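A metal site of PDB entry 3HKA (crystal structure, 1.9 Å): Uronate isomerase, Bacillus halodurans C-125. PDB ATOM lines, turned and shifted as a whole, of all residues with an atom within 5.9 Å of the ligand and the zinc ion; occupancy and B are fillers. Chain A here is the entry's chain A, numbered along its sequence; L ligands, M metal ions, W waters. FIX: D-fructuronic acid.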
ATOM      1  N   HIS A  26      -8.626 -17.804  13.520  1.00  0.00           N
ATOM      2  CA  HIS A  26      -9.164 -18.270  14.797  1.00  0.00           C
ATOM      3  C   HIS A  26      -9.944 -19.569  14.669  1.00  0.00           C
ATOM      4  O   HIS A  26     -11.026 -19.599  14.091  1.00  0.00           O
ATOM      5  CB  HIS A  26     -10.053 -17.246  15.513  1.00  0.00           C
ATOM      6  CG  HIS A  26     -10.646 -17.789  16.780  1.00  0.00           C
ATOM      7  ND1 HIS A  26      -9.875 -18.294  17.809  1.00  0.00           N
ATOM      8  CD2 HIS A  26     -11.937 -17.996  17.140  1.00  0.00           C
ATOM      9  CE1 HIS A  26     -10.665 -18.794  18.748  1.00  0.00           C
ATOM     10  NE2 HIS A  26     -11.917 -18.624  18.364  1.00  0.00           N
ATOM     11  N   THR A  27      -9.382 -20.641  15.216  1.00  0.00           N
ATOM     12  CA  THR A  27     -10.034 -21.940  15.186  1.00  0.00           C
ATOM     13  C   THR A  27      -9.698 -22.651  16.490  1.00  0.00           C
ATOM     14  O   THR A  27      -8.911 -22.151  17.296  1.00  0.00           O
ATOM     15  CB  THR A  27      -9.510 -22.852  14.054  1.00  0.00           C
ATOM     16  OG1 THR A  27      -8.262 -23.441  14.449  1.00  0.00           O
ATOM     17  CG2 THR A  27      -9.316 -22.050  12.769  1.00  0.00           C
ATOM     18  N   HIS A  28     -10.294 -23.819  16.654  1.00  0.00           N
ATOM     19  CA  HIS A  28     -10.043 -24.637  17.819  1.00  0.00           C
ATOM     20  C   HIS A  28      -9.513 -25.980  17.311  1.00  0.00           C
ATOM     21  O   HIS A  28      -9.862 -27.050  17.808  1.00  0.00           O
ATOM     22  CB  HIS A  28     -11.342 -24.823  18.615  1.00  0.00           C
ATOM     23  CG  HIS A  28     -11.780 -23.560  19.298  1.00  0.00           C
ATOM     24  ND1 HIS A  28     -11.306 -23.189  20.543  1.00  0.00           N
ATOM     25  CD2 HIS A  28     -12.592 -22.567  18.894  1.00  0.00           C
ATOM     26  CE1 HIS A  28     -11.809 -22.020  20.863  1.00  0.00           C
ATOM     27  NE2 HIS A  28     -12.589 -21.611  19.879  1.00  0.00           N
ATOM     28  N   TYR A  48     -20.953 -31.748  17.499  1.00  0.00           N
ATOM     29  CA  TYR A  48     -20.493 -30.359  17.658  1.00  0.00           C
ATOM     30  C   TYR A  48     -21.482 -29.760  18.658  1.00  0.00           C
ATOM     31  O   TYR A  48     -22.670 -30.011  18.559  1.00  0.00           O
ATOM     32  CB  TYR A  48     -20.613 -29.679  16.288  1.00  0.00           C
ATOM     33  CG  TYR A  48     -20.238 -28.218  16.179  1.00  0.00           C
ATOM     34  CD1 TYR A  48     -19.132 -27.698  16.850  1.00  0.00           C
ATOM     35  CD2 TYR A  48     -20.916 -27.396  15.294  1.00  0.00           C
ATOM     36  CE1 TYR A  48     -18.715 -26.380  16.626  1.00  0.00           C
ATOM     37  CE2 TYR A  48     -20.511 -26.081  15.050  1.00  0.00           C
ATOM     38  CZ  TYR A  48     -19.406 -25.583  15.720  1.00  0.00           C
ATOM     39  OH  TYR A  48     -19.000 -24.298  15.454  1.00  0.00           O
ATOM     40  N   HIS A  49     -21.003 -28.972  19.629  1.00  0.00           N
ATOM     41  CA  HIS A  49     -21.942 -28.438  20.618  1.00  0.00           C
ATOM     42  C   HIS A  49     -23.119 -27.638  20.069  1.00  0.00           C
ATOM     43  O   HIS A  49     -24.171 -27.590  20.703  1.00  0.00           O
ATOM     44  CB  HIS A  49     -21.211 -27.695  21.760  1.00  0.00           C
ATOM     45  CG  HIS A  49     -20.681 -26.336  21.405  1.00  0.00           C
ATOM     46  ND1 HIS A  49     -21.498 -25.240  21.221  1.00  0.00           N
ATOM     47  CD2 HIS A  49     -19.409 -25.891  21.276  1.00  0.00           C
ATOM     48  CE1 HIS A  49     -20.746 -24.165  21.013  1.00  0.00           C
ATOM     49  NE2 HIS A  49     -19.479 -24.538  21.038  1.00  0.00           N
ATOM     50  N   TYR A  50     -22.965 -27.050  18.884  1.00  0.00           N
ATOM     51  CA  TYR A  50     -24.070 -26.300  18.283  1.00  0.00           C
ATOM     52  C   TYR A  50     -25.249 -27.247  18.093  1.00  0.00           C
ATOM     53  O   TYR A  50     -26.406 -26.880  18.318  1.00  0.00           O
ATOM     54  CB  TYR A  50     -23.686 -25.777  16.896  1.00  0.00           C
ATOM     55  CG  TYR A  50     -22.877 -24.494  16.888  1.00  0.00           C
ATOM     56  CD1 TYR A  50     -21.844 -24.293  17.786  1.00  0.00           C
ATOM     57  CD2 TYR A  50     -23.099 -23.532  15.902  1.00  0.00           C
ATOM     58  CE1 TYR A  50     -21.038 -23.166  17.707  1.00  0.00           C
ATOM     59  CE2 TYR A  50     -22.308 -22.399  15.814  1.00  0.00           C
ATOM     60  CZ  TYR A  50     -21.274 -22.221  16.721  1.00  0.00           C
ATOM     61  OH  TYR A  50     -20.456 -21.129  16.608  1.00  0.00           O
ATOM     62  N   THR A 143      -5.976 -22.203  19.015  1.00  0.00           N
ATOM     63  CA  THR A 143      -6.292 -21.569  20.285  1.00  0.00           C
ATOM     64  C   THR A 143      -5.493 -22.426  21.256  1.00  0.00           C
ATOM     65  O   THR A 143      -5.887 -23.550  21.582  1.00  0.00           O
ATOM     66  CB  THR A 143      -7.776 -21.660  20.635  1.00  0.00           C
ATOM     67  OG1 THR A 143      -8.542 -20.900  19.684  1.00  0.00           O
ATOM     68  CG2 THR A 143      -8.027 -21.124  22.042  1.00  0.00           C
ATOM     69  N   ARG A 170      -3.871 -18.290  24.336  1.00  0.00           N
ATOM     70  CA  ARG A 170      -5.181 -18.055  24.952  1.00  0.00           C
ATOM     71  C   ARG A 170      -4.991 -17.935  26.472  1.00  0.00           C
ATOM     72  O   ARG A 170      -4.378 -18.808  27.089  1.00  0.00           O
ATOM     73  CB  ARG A 170      -6.130 -19.204  24.612  1.00  0.00           C
ATOM     74  CG  ARG A 170      -7.570 -18.979  25.039  1.00  0.00           C
ATOM     75  CD  ARG A 170      -8.168 -17.716  24.409  1.00  0.00           C
ATOM     76  NE  ARG A 170      -9.571 -17.612  24.783  1.00  0.00           N
ATOM     77  CZ  ARG A 170     -10.583 -17.969  23.992  1.00  0.00           C
ATOM     78  NH1 ARG A 170     -10.351 -18.426  22.774  1.00  0.00           N
ATOM     79  NH2 ARG A 170     -11.816 -17.913  24.455  1.00  0.00           N
ATOM     80  N   ASP A 172      -7.746 -16.918  28.968  1.00  0.00           N
ATOM     81  CA  ASP A 172      -8.956 -16.774  29.788  1.00  0.00           C
ATOM     82  C   ASP A 172      -8.768 -17.110  31.276  1.00  0.00           C
ATOM     83  O   ASP A 172      -9.190 -16.355  32.153  1.00  0.00           O
ATOM     84  CB  ASP A 172     -10.088 -17.622  29.207  1.00  0.00           C
ATOM     85  CG  ASP A 172     -10.584 -17.075  27.878  1.00  0.00           C
ATOM     86  OD1 ASP A 172      -9.764 -16.508  27.132  1.00  0.00           O
ATOM     87  OD2 ASP A 172     -11.791 -17.245  27.576  1.00  0.00           O
ATOM     88  N   SER A 223     -11.460 -14.274  25.815  1.00  0.00           N
ATOM     89  CA  SER A 223     -12.869 -14.050  25.523  1.00  0.00           C
ATOM     90  C   SER A 223     -13.357 -13.347  26.787  1.00  0.00           C
ATOM     91  O   SER A 223     -12.935 -13.691  27.885  1.00  0.00           O
ATOM     92  CB  SER A 223     -13.624 -15.379  25.279  1.00  0.00           C
ATOM     93  OG  SER A 223     -13.766 -16.147  26.461  1.00  0.00           O
ATOM     94  N   MET A 258     -12.345 -11.166  22.412  1.00  0.00           N
ATOM     95  CA  MET A 258     -13.597 -11.678  21.879  1.00  0.00           C
ATOM     96  C   MET A 258     -14.598 -11.359  22.991  1.00  0.00           C
ATOM     97  O   MET A 258     -14.712 -12.072  23.991  1.00  0.00           O
ATOM     98  CB  MET A 258     -13.472 -13.177  21.607  1.00  0.00           C
ATOM     99  CG  MET A 258     -12.193 -13.495  20.848  1.00  0.00           C
ATOM    100  SD  MET A 258     -12.233 -15.016  19.887  1.00  0.00           S
ATOM    101  CE  MET A 258     -11.777 -16.177  21.085  1.00  0.00           C
ATOM    102  N   LYS A 263     -20.630 -16.886  30.092  1.00  0.00           N
ATOM    103  CA  LYS A 263     -20.351 -18.300  30.303  1.00  0.00           C
ATOM    104  C   LYS A 263     -21.296 -19.079  31.199  1.00  0.00           C
ATOM    105  O   LYS A 263     -21.783 -18.576  32.217  1.00  0.00           O
ATOM    106  CB  LYS A 263     -18.929 -18.451  30.861  1.00  0.00           C
ATOM    107  CG  LYS A 263     -17.835 -17.861  29.976  1.00  0.00           C
ATOM    108  CD  LYS A 263     -17.713 -18.591  28.639  1.00  0.00           C
ATOM    109  CE  LYS A 263     -17.099 -19.977  28.795  1.00  0.00           C
ATOM    110  NZ  LYS A 263     -16.896 -20.641  27.465  1.00  0.00           N
ATOM    111  N   ASP A 271     -20.204 -27.162  26.871  1.00  0.00           N
ATOM    112  CA  ASP A 271     -19.807 -26.138  25.912  1.00  0.00           C
ATOM    113  C   ASP A 271     -20.974 -25.526  25.147  1.00  0.00           C
ATOM    114  O   ASP A 271     -20.806 -24.530  24.443  1.00  0.00           O
ATOM    115  CB  ASP A 271     -18.799 -26.683  24.894  1.00  0.00           C
ATOM    116  CG  ASP A 271     -17.449 -27.013  25.508  1.00  0.00           C
ATOM    117  OD1 ASP A 271     -17.125 -26.455  26.571  1.00  0.00           O
ATOM    118  OD2 ASP A 271     -16.720 -27.824  24.906  1.00  0.00           O
ATOM    119  N   ASP A 274     -23.314 -21.651  26.862  1.00  0.00           N
ATOM    120  CA  ASP A 274     -22.911 -20.245  26.948  1.00  0.00           C
ATOM    121  C   ASP A 274     -23.946 -19.346  26.259  1.00  0.00           C
ATOM    122  O   ASP A 274     -24.594 -19.745  25.283  1.00  0.00           O
ATOM    123  CB  ASP A 274     -21.528 -20.022  26.327  1.00  0.00           C
ATOM    124  CG  ASP A 274     -20.419 -20.754  27.070  1.00  0.00           C
ATOM    125  OD1 ASP A 274     -20.527 -20.934  28.299  1.00  0.00           O
ATOM    126  OD2 ASP A 274     -19.410 -21.134  26.417  1.00  0.00           O
ATOM    127  N   TRP A 325     -18.413 -13.941  14.696  1.00  0.00           N
ATOM    128  CA  TRP A 325     -18.296 -14.893  15.775  1.00  0.00           C
ATOM    129  C   TRP A 325     -19.510 -15.587  16.374  1.00  0.00           C
ATOM    130  O   TRP A 325     -20.484 -14.955  16.779  1.00  0.00           O
ATOM    131  CB  TRP A 325     -17.502 -14.198  16.906  1.00  0.00           C
ATOM    132  CG  TRP A 325     -17.117 -15.077  18.052  1.00  0.00           C
ATOM    133  CD1 TRP A 325     -16.699 -16.380  18.003  1.00  0.00           C
ATOM    134  CD2 TRP A 325     -17.027 -14.678  19.432  1.00  0.00           C
ATOM    135  NE1 TRP A 325     -16.336 -16.811  19.254  1.00  0.00           N
ATOM    136  CE2 TRP A 325     -16.532 -15.788  20.155  1.00  0.00           C
ATOM    137  CE3 TRP A 325     -17.302 -13.488  20.122  1.00  0.00           C
ATOM    138  CZ2 TRP A 325     -16.313 -15.738  21.537  1.00  0.00           C
ATOM    139  CZ3 TRP A 325     -17.084 -13.438  21.493  1.00  0.00           C
ATOM    140  CH2 TRP A 325     -16.593 -14.568  22.186  1.00  0.00           C
ATOM    141  N   TRP A 326     -19.436 -16.914  16.402  1.00  0.00           N
ATOM    142  CA  TRP A 326     -20.447 -17.737  17.060  1.00  0.00           C
ATOM    143  C   TRP A 326     -21.906 -17.498  16.644  1.00  0.00           C
ATOM    144  O   TRP A 326     -22.324 -17.873  15.544  1.00  0.00           O
ATOM    145  CB  TRP A 326     -20.284 -17.462  18.555  1.00  0.00           C
ATOM    146  CG  TRP A 326     -20.628 -18.561  19.503  1.00  0.00           C
ATOM    147  CD1 TRP A 326     -21.529 -19.566  19.319  1.00  0.00           C
ATOM    148  CD2 TRP A 326     -20.135 -18.696  20.841  1.00  0.00           C
ATOM    149  NE1 TRP A 326     -21.629 -20.335  20.475  1.00  0.00           N
ATOM    150  CE2 TRP A 326     -20.784 -19.815  21.418  1.00  0.00           C
ATOM    151  CE3 TRP A 326     -19.205 -17.977  21.606  1.00  0.00           C
ATOM    152  CZ2 TRP A 326     -20.522 -20.231  22.731  1.00  0.00           C
ATOM    153  CZ3 TRP A 326     -18.952 -18.397  22.920  1.00  0.00           C
ATOM    154  CH2 TRP A 326     -19.615 -19.517  23.458  1.00  0.00           C
ATOM    155  N   HIS A 353     -13.641 -15.933  10.123  1.00  0.00           N
ATOM    156  CA  HIS A 353     -12.793 -16.983  10.670  1.00  0.00           C
ATOM    157  C   HIS A 353     -13.770 -18.150  10.846  1.00  0.00           C
ATOM    158  O   HIS A 353     -14.985 -17.930  10.916  1.00  0.00           O
ATOM    159  CB  HIS A 353     -12.153 -16.575  12.010  1.00  0.00           C
ATOM    160  CG  HIS A 353     -13.124 -16.420  13.137  1.00  0.00           C
ATOM    161  ND1 HIS A 353     -13.761 -15.226  13.414  1.00  0.00           N
ATOM    162  CD2 HIS A 353     -13.533 -17.295  14.078  1.00  0.00           C
ATOM    163  CE1 HIS A 353     -14.527 -15.382  14.476  1.00  0.00           C
ATOM    164  NE2 HIS A 353     -14.403 -16.624  14.898  1.00  0.00           N
ATOM    165  N   SER A 354     -13.266 -19.375  10.915  1.00  0.00           N
ATOM    166  CA  SER A 354     -14.164 -20.535  11.032  1.00  0.00           C
ATOM    167  C   SER A 354     -14.526 -20.953  12.445  1.00  0.00           C
ATOM    168  O   SER A 354     -15.629 -21.439  12.693  1.00  0.00           O
ATOM    169  CB  SER A 354     -13.560 -21.734  10.315  1.00  0.00           C
ATOM    170  OG  SER A 354     -12.455 -22.236  11.035  1.00  0.00           O
ATOM    171  N   ASP A 355     -13.598 -20.780  13.383  1.00  0.00           N
ATOM    172  CA  ASP A 355     -13.823 -21.191  14.761  1.00  0.00           C
ATOM    173  C   ASP A 355     -14.031 -22.701  14.777  1.00  0.00           C
ATOM    174  O   ASP A 355     -14.637 -23.252  15.692  1.00  0.00           O
ATOM    175  CB  ASP A 355     -15.084 -20.524  15.321  1.00  0.00           C
ATOM    176  CG  ASP A 355     -14.818 -19.813  16.633  1.00  0.00           C
ATOM    177  OD1 ASP A 355     -14.190 -20.417  17.529  1.00  0.00           O
ATOM    178  OD2 ASP A 355     -15.239 -18.641  16.763  1.00  0.00           O
ATOM    179  N   ARG A 357     -13.998 -26.458  15.342  1.00  0.00           N
ATOM    180  CA  ARG A 357     -13.670 -27.306  16.486  1.00  0.00           C
ATOM    181  C   ARG A 357     -13.420 -28.711  15.955  1.00  0.00           C
ATOM    182  O   ARG A 357     -12.700 -29.505  16.565  1.00  0.00           O
ATOM    183  CB  ARG A 357     -14.822 -27.312  17.491  1.00  0.00           C
ATOM    184  CG  ARG A 357     -14.794 -26.138  18.469  1.00  0.00           C
ATOM    185  CD  ARG A 357     -16.021 -26.142  19.371  1.00  0.00           C
ATOM    186  NE  ARG A 357     -15.911 -25.163  20.447  1.00  0.00           N
ATOM    187  CZ  ARG A 357     -15.092 -25.299  21.487  1.00  0.00           C
ATOM    188  NH1 ARG A 357     -14.315 -26.368  21.587  1.00  0.00           N
ATOM    189  NH2 ARG A 357     -15.050 -24.365  22.426  1.00  0.00           N
ATOM    190  N   LYS A 365     -17.626 -24.062   6.827  1.00  0.00           N
ATOM    191  CA  LYS A 365     -17.431 -22.722   7.375  1.00  0.00           C
ATOM    192  C   LYS A 365     -17.005 -21.766   6.266  1.00  0.00           C
ATOM    193  O   LYS A 365     -17.637 -20.721   6.068  1.00  0.00           O
ATOM    194  CB  LYS A 365     -16.364 -22.738   8.476  1.00  0.00           C
ATOM    195  CG  LYS A 365     -16.759 -23.512   9.725  1.00  0.00           C
ATOM    196  CD  LYS A 365     -17.769 -22.764  10.586  1.00  0.00           C
ATOM    197  CE  LYS A 365     -17.982 -23.491  11.909  1.00  0.00           C
ATOM    198  NZ  LYS A 365     -19.034 -22.871  12.776  1.00  0.00           N
HETATM  199  O1A FIX L   1     -12.950 -19.087  21.259  1.00  0.00           O
HETATM  200  C1  FIX L   1     -13.946 -19.043  22.028  1.00  0.00           C
HETATM  201  O1B FIX L   1     -13.922 -18.726  23.228  1.00  0.00           O
HETATM  202  C2  FIX L   1     -15.314 -19.399  21.428  1.00  0.00           C
HETATM  203  O2  FIX L   1     -15.266 -19.243  20.001  1.00  0.00           O
HETATM  204  C3  FIX L   1     -15.718 -20.841  21.823  1.00  0.00           C
HETATM  205  O3  FIX L   1     -15.725 -20.938  23.270  1.00  0.00           O
HETATM  206  C4  FIX L   1     -17.116 -21.333  21.348  1.00  0.00           C
HETATM  207  O4  FIX L   1     -17.491 -22.535  22.040  1.00  0.00           O
HETATM  208  C5  FIX L   1     -17.176 -21.603  19.812  1.00  0.00           C
HETATM  209  O5  FIX L   1     -16.202 -22.070  19.217  1.00  0.00           O
HETATM  210  C6  FIX L   1     -18.448 -21.308  19.036  1.00  0.00           C
HETATM  211  O6  FIX L   1     -18.183 -21.087  17.661  1.00  0.00           O
HETATM  212 ZN    ZN M   1     -13.446 -19.735  19.321  1.00  0.00          ZN
HETATM  213  O   HOH W   1     -15.652 -18.205  25.463  1.00  0.00           O
HETATM  214  O   HOH W   2     -16.997 -23.550  16.960  1.00  0.00           O
HETATM  215  O   HOH W   3     -18.754 -20.632  14.347  1.00  0.00           O
HETATM  216  O   HOH W   4     -13.116 -21.843  25.035  1.00  0.00           O
HETATM  217  O   HOH W   5     -18.728 -22.657  24.367  1.00  0.00           O
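An oxygen (O6) of the ligand sits at hydrogen-bond distance from the side-chain hydroxyl (OH) of Tyr 50, at 2.5 Å. The guanidinium group (NH2) of Arg 170 is in salt-bridge range of an oxygen (O1B) of the ligand (2.6 Å). The indole nitrogen (NE1) of Trp 325 lies close to an oxygen (O2) of the ligand (2.8 Å). NE2 of His 49 lies within hydrogen-bond range of O4 of the ligand (3.0 Å). NH2 of Arg 357 is in hydrogen-bond range of O4 of the ligand, at 3.1 Å.
The indole nitrogen of Trp 325 sits close to the side-chain carboxylate of Asp 355 (3.3 Å). OD2 of Asp 355 lies within hydrogen-bond range of NE2 of His 353, 2.9 Å away. A ring nitrogen (ND1) of His 26 sits close to the side-chain hydroxyl of Thr 143 (3.5 Å). The guanidinium group (NH2) of Arg 170 lies close to the side-chain hydroxyl (OG) of Ser 223, 3.3 Å away. OD1 of Asp 172 is in salt-bridge range of NE of Arg 170 (2.6 Å). ND1 of His 49 sits at hydrogen-bond distance from O of Asp 271 (3.4 Å). OG of Ser 223 sits at hydrogen-bond distance from OD2 of Asp 172, at 2.5 Å. NZ of Lys 365 sits at hydrogen-bond distance from OH of Tyr 48, 3.0 Å away.
Tyr 48 touches the ligand (OH to O6, 3.98 Å). CB of Ser 223 touches O1B of the ligand, at 3.9 Å. Met 258 touches the ligand. CG of Trp 326 touches C6 of the ligand (3.5 Å). Hydrophobic or aromatic side chains within 4 Å of the ligand: His 26, His 28, His 49, Tyr 50, Met 258, Trp 325 and Trp 326. Of the 21 residues printed, 12 come within 4 Å of the ligand. The nearest printed residue that does not touch the ligand is Lys 263 (4.4 Å).
Within 4 Å of the zinc ion: His 26, His 28 and Asp 355.
The zinc ion is bound by an oxygen (O2) of the ligand, the side-chain carboxylate of Asp 355, an oxygen (O1A) of the ligand, a ring nitrogen (NE2) of His 26 and a ring nitrogen (NE2) of His 28.
Water W5 lies within hydrogen-bond range of O4 of the ligand (2.6 Å), OD2 of Asp 274 (2.6 Å) and O of Asp 271 (2.8 Å). Water W2 lies within hydrogen-bond range of the side-chain hydroxyl (OH) of Tyr 48, the backbone carbonyl oxygen (O) of Asp 355 and an oxygen (O5) of the ligand. Water W1 lies within hydrogen-bond range of O1B of the ligand (2.9 Å), OG of Ser 223 (3.0 Å) and NZ of Lys 263 (3.4 Å). Water W3 lies within hydrogen-bond range of NZ of Lys 365 (2.7 Å), OH of Tyr 50 (2.9 Å) and O6 of the ligand (3.4 Å).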
